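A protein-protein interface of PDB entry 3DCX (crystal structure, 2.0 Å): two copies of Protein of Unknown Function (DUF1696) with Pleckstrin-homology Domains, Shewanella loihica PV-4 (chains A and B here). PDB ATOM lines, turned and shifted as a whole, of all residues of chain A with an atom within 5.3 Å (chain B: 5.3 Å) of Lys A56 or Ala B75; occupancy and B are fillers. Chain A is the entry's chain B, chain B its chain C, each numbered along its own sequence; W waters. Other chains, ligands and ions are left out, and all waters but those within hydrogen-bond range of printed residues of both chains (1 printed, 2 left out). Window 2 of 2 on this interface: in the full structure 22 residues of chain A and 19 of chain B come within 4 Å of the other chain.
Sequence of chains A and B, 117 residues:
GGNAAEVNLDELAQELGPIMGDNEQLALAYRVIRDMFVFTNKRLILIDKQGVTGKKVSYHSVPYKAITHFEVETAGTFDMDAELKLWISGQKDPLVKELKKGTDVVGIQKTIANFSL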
ATOM      1  N   ASP A  48      -6.207 -14.556 -26.578  1.00  0.00           N
ATOM      2  CA  ASP A  48      -5.229 -14.827 -27.610  1.00  0.00           C
ATOM      3  C   ASP A  48      -4.007 -13.968 -27.367  1.00  0.00           C
ATOM      4  O   ASP A  48      -4.136 -12.774 -27.116  1.00  0.00           O
ATOM      5  CB  ASP A  48      -5.796 -14.494 -28.993  1.00  0.00           C
ATOM      6  CG  ASP A  48      -6.759 -15.564 -29.527  1.00  0.00           C
ATOM      7  OD1 ASP A  48      -7.184 -16.495 -28.777  1.00  0.00           O
ATOM      8  OD2 ASP A  48      -7.093 -15.477 -30.730  1.00  0.00           O
ATOM      9  N   LYS A  49      -2.830 -14.586 -27.456  1.00  0.00           N
ATOM     10  CA  LYS A  49      -1.560 -13.880 -27.348  1.00  0.00           C
ATOM     11  C   LYS A  49      -0.812 -13.887 -28.689  1.00  0.00           C
ATOM     12  O   LYS A  49      -0.864 -14.864 -29.428  1.00  0.00           O
ATOM     13  CB  LYS A  49      -0.729 -14.501 -26.250  1.00  0.00           C
ATOM     14  CG  LYS A  49      -1.481 -14.606 -24.957  1.00  0.00           C
ATOM     15  CD  LYS A  49      -0.570 -14.769 -23.790  1.00  0.00           C
ATOM     16  CE  LYS A  49      -1.306 -14.670 -22.464  1.00  0.00           C
ATOM     17  NZ  LYS A  49      -0.331 -14.635 -21.352  1.00  0.00           N
ATOM     18  N   GLN A  50      -0.142 -12.775 -28.990  1.00  0.00           N
ATOM     19  CA  GLN A  50       0.580 -12.577 -30.239  1.00  0.00           C
ATOM     20  C   GLN A  50       2.037 -12.244 -29.965  1.00  0.00           C
ATOM     21  O   GLN A  50       2.340 -11.541 -29.006  1.00  0.00           O
ATOM     22  CB  GLN A  50      -0.044 -11.423 -31.022  1.00  0.00           C
ATOM     23  CG  GLN A  50      -1.135 -11.847 -31.998  1.00  0.00           C
ATOM     24  CD  GLN A  50      -1.918 -10.661 -32.540  1.00  0.00           C
ATOM     25  OE1 GLN A  50      -2.608  -9.956 -31.791  1.00  0.00           O
ATOM     26  NE2 GLN A  50      -1.817 -10.435 -33.845  1.00  0.00           N
ATOM     27  N   THR A  53       6.846 -13.040 -27.370  1.00  0.00           N
ATOM     28  CA  THR A  53       6.734 -12.785 -25.918  1.00  0.00           C
ATOM     29  C   THR A  53       5.324 -12.974 -25.431  1.00  0.00           C
ATOM     30  O   THR A  53       5.106 -13.159 -24.234  1.00  0.00           O
ATOM     31  CB  THR A  53       7.162 -11.339 -25.501  1.00  0.00           C
ATOM     32  OG1 THR A  53       6.341 -10.368 -26.175  1.00  0.00           O
ATOM     33  CG2 THR A  53       8.653 -11.093 -25.829  1.00  0.00           C
ATOM     34  N   GLY A  54       4.365 -12.906 -26.354  1.00  0.00           N
ATOM     35  CA  GLY A  54       2.972 -12.936 -25.999  1.00  0.00           C
ATOM     36  C   GLY A  54       2.512 -11.703 -25.250  1.00  0.00           C
ATOM     37  O   GLY A  54       1.539 -11.787 -24.481  1.00  0.00           O
ATOM     38  N   LYS A  55       3.185 -10.571 -25.473  1.00  0.00           N
ATOM     39  CA  LYS A  55       2.872  -9.338 -24.773  1.00  0.00           C
ATOM     40  C   LYS A  55       1.582  -8.721 -25.294  1.00  0.00           C
ATOM     41  O   LYS A  55       0.892  -8.018 -24.564  1.00  0.00           O
ATOM     42  CB  LYS A  55       4.036  -8.332 -24.838  1.00  0.00           C
ATOM     43  CG  LYS A  55       4.219  -7.579 -26.171  1.00  0.00           C
ATOM     44  CD  LYS A  55       5.434  -6.599 -26.181  1.00  0.00           C
ATOM     45  CE  LYS A  55       5.423  -5.741 -27.433  1.00  0.00           C
ATOM     46  NZ  LYS A  55       6.572  -4.776 -27.588  1.00  0.00           N
ATOM     47  N   LYS A  56       1.267  -8.967 -26.556  1.00  0.00           N
ATOM     48  CA  LYS A  56       0.034  -8.428 -27.163  1.00  0.00           C
ATOM     49  C   LYS A  56      -1.130  -9.414 -26.937  1.00  0.00           C
ATOM     50  O   LYS A  56      -1.126 -10.503 -27.473  1.00  0.00           O
ATOM     51  CB  LYS A  56       0.264  -8.186 -28.659  1.00  0.00           C
ATOM     52  CG  LYS A  56      -0.679  -7.187 -29.300  1.00  0.00           C
ATOM     53  CD  LYS A  56      -0.591  -7.273 -30.803  1.00  0.00           C
ATOM     54  CE  LYS A  56      -1.515  -6.276 -31.476  1.00  0.00           C
ATOM     55  NZ  LYS A  56      -1.664  -6.565 -32.940  1.00  0.00           N
ATOM     56  N   VAL A  57      -2.094  -9.030 -26.102  1.00  0.00           N
ATOM     57  CA  VAL A  57      -3.125  -9.942 -25.651  1.00  0.00           C
ATOM     58  C   VAL A  57      -4.491  -9.376 -26.007  1.00  0.00           C
ATOM     59  O   VAL A  57      -4.741  -8.193 -25.797  1.00  0.00           O
ATOM     60  CB  VAL A  57      -3.085 -10.134 -24.125  1.00  0.00           C
ATOM     61  CG1 VAL A  57      -4.179 -11.105 -23.677  1.00  0.00           C
ATOM     62  CG2 VAL A  57      -1.738 -10.635 -23.674  1.00  0.00           C
ATOM     63  N   SER A  58      -5.360 -10.236 -26.531  1.00  0.00           N
ATOM     64  CA  SER A  58      -6.749  -9.864 -26.757  1.00  0.00           C
ATOM     65  C   SER A  58      -7.688 -10.782 -25.991  1.00  0.00           C
ATOM     66  O   SER A  58      -7.454 -12.007 -25.884  1.00  0.00           O
ATOM     67  CB  SER A  58      -7.099  -9.839 -28.253  1.00  0.00           C
ATOM     68  OG  SER A  58      -6.599 -10.975 -28.919  1.00  0.00           O
ATOM     69  N   GLU B  73      -8.042  -5.409 -26.789  1.00  0.00           N
ATOM     70  CA  GLU B  73      -6.671  -5.800 -27.105  1.00  0.00           C
ATOM     71  C   GLU B  73      -5.704  -4.787 -26.531  1.00  0.00           C
ATOM     72  O   GLU B  73      -5.913  -3.597 -26.697  1.00  0.00           O
ATOM     73  CB  GLU B  73      -6.497  -5.834 -28.610  1.00  0.00           C
ATOM     74  CG  GLU B  73      -5.159  -6.345 -29.060  1.00  0.00           C
ATOM     75  CD  GLU B  73      -5.149  -6.615 -30.539  1.00  0.00           C
ATOM     76  OE1 GLU B  73      -5.669  -5.762 -31.290  1.00  0.00           O
ATOM     77  OE2 GLU B  73      -4.649  -7.692 -30.934  1.00  0.00           O
ATOM     78  N   THR B  74      -4.658  -5.263 -25.857  1.00  0.00           N
ATOM     79  CA  THR B  74      -3.624  -4.408 -25.255  1.00  0.00           C
ATOM     80  C   THR B  74      -2.267  -4.601 -25.926  1.00  0.00           C
ATOM     81  O   THR B  74      -1.879  -5.736 -26.214  1.00  0.00           O
ATOM     82  CB  THR B  74      -3.444  -4.767 -23.760  1.00  0.00           C
ATOM     83  OG1 THR B  74      -4.732  -4.769 -23.114  1.00  0.00           O
ATOM     84  CG2 THR B  74      -2.467  -3.763 -23.044  1.00  0.00           C
ATOM     85  N   ALA B  75      -1.529  -3.493 -26.080  1.00  0.00           N
ATOM     86  CA  ALA B  75      -0.237  -3.435 -26.814  1.00  0.00           C
ATOM     87  C   ALA B  75       0.873  -4.263 -26.160  1.00  0.00           C
ATOM     88  O   ALA B  75       1.622  -4.989 -26.833  1.00  0.00           O
ATOM     89  CB  ALA B  75       0.231  -1.966 -26.981  1.00  0.00           C
ATOM     90  N   GLY B  76       0.959  -4.185 -24.837  1.00  0.00           N
ATOM     91  CA  GLY B  76       2.041  -4.849 -24.152  1.00  0.00           C
ATOM     92  C   GLY B  76       1.759  -5.353 -22.759  1.00  0.00           C
ATOM     93  O   GLY B  76       0.636  -5.279 -22.233  1.00  0.00           O
ATOM     94  N   THR B  77       2.815  -5.909 -22.188  1.00  0.00           N
ATOM     95  CA  THR B  77       2.824  -6.337 -20.809  1.00  0.00           C
ATOM     96  C   THR B  77       2.891  -5.103 -19.891  1.00  0.00           C
ATOM     97  O   THR B  77       2.170  -5.051 -18.881  1.00  0.00           O
ATOM     98  CB  THR B  77       4.018  -7.285 -20.558  1.00  0.00           C
ATOM     99  OG1 THR B  77       3.758  -8.556 -21.181  1.00  0.00           O
ATOM    100  CG2 THR B  77       4.238  -7.461 -19.083  1.00  0.00           C
ATOM    101  N   ASP B  79       3.198  -1.761 -21.609  1.00  0.00           N
ATOM    102  CA  ASP B  79       2.635  -0.711 -22.436  1.00  0.00           C
ATOM    103  C   ASP B  79       1.127  -0.914 -22.447  1.00  0.00           C
ATOM    104  O   ASP B  79       0.599  -1.865 -23.060  1.00  0.00           O
ATOM    105  CB  ASP B  79       3.200  -0.785 -23.857  1.00  0.00           C
ATOM    106  CG  ASP B  79       2.524   0.180 -24.810  1.00  0.00           C
ATOM    107  OD1 ASP B  79       1.421   0.643 -24.488  1.00  0.00           O
ATOM    108  OD2 ASP B  79       3.108   0.482 -25.871  1.00  0.00           O
ATOM    109  N   ASP B  81      -1.479   0.871 -23.523  1.00  0.00           N
ATOM    110  CA  ASP B  81      -2.454   1.333 -24.508  1.00  0.00           C
ATOM    111  C   ASP B  81      -3.313   0.134 -24.881  1.00  0.00           C
ATOM    112  O   ASP B  81      -2.841  -1.005 -24.857  1.00  0.00           O
ATOM    113  CB  ASP B  81      -1.830   1.958 -25.750  1.00  0.00           C
ATOM    114  CG  ASP B  81      -1.080   3.241 -25.451  1.00  0.00           C
ATOM    115  OD1 ASP B  81      -1.313   3.848 -24.372  1.00  0.00           O
ATOM    116  OD2 ASP B  81      -0.261   3.633 -26.315  1.00  0.00           O
ATOM    117  N   ALA B  82      -4.578   0.401 -25.200  1.00  0.00           N
ATOM    118  CA  ALA B  82      -5.539  -0.630 -25.482  1.00  0.00           C
ATOM    119  C   ALA B  82      -6.582  -0.106 -26.439  1.00  0.00           C
ATOM    120  O   ALA B  82      -6.793   1.114 -26.558  1.00  0.00           O
ATOM    121  CB  ALA B  82      -6.220  -1.160 -24.165  1.00  0.00           C
HETATM  122  O   HOH W   1      -5.997  -7.032 -22.973  1.00  0.00           O
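Along chain B the printed residues that touch a printed residue of chain A span positions 73 to 77.
Of the 9 printed residues of chain A, 4 touch a printed residue of chain B.
Among the printed residues, 10 pairs touch across the chains.
The backbone carbonyl oxygen of Lys A56 sits at hydrogen-bond distance from the backbone NH of Gln A50.
The backbone NH of Ala B75 is in hydrogen-bond range of the backbone carbonyl oxygen of Asp B81 (3.1 Å).
OG1 of Thr A53 lies close to N of Lys A55, 3.2 Å away.
The backbone carbonyl oxygen (O) of Val A57 sits at hydrogen-bond distance from the backbone NH (N) of Thr B74 (2.9 Å).
The side-chain amino group of Lys A56 lies within salt-bridge range of the side-chain carboxylate of Glu B73 (3.8 Å).
The side-chain carboxylate (OE2) of Glu B73 sits close to the side-chain amide oxygen (OE1) of Gln A50 (3.2 Å).
Lys A49 touches none of the printed residues of chain B.
Of the printed residues of chain B, Gln A50 touches Glu B73 (3.2 Å).
Of the printed residues of chain B, Lys A55 touches Thr B74, Ala B75, Gly B76 and Thr B77.
Lys A56 touches just these residues of chain B: Glu B73 (3.5 Å), Thr B74 (3.4 Å) and Ala B75 (3.8 Å).
Of the printed residues of chain B, Val A57 touches Glu B73 and Thr B74.
Of the printed residues of chain A, Glu B73 touches Gln A50 (3.2 Å), Lys A56 (3.5 Å) and Val A57 (3.3 Å).
Printed residues of chain A within 4 Å of Ala B75: Lys A55 and Lys A56.
The nearest printed residue of chain A that does not touch Ala B75 is Val A57 (5.5 Å).
No position is printed for both chains.
Among the printed residues, merely in contact across the chains: Lys A55 with Gly B76 (3.3 Å), Val A57 with Glu B73 (3.3 Å), Lys A56 with Thr B74 (3.4 Å), Lys A55 with Thr B77 (3.7 Å), Lys A55 with Ala B75 (3.7 Å), Lys A56 with Ala B75 (3.8 Å) and Lys A55 with Thr B74 (3.95 Å).
Water W1 bridges OG1 of Thr B74 and O of Val A57.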
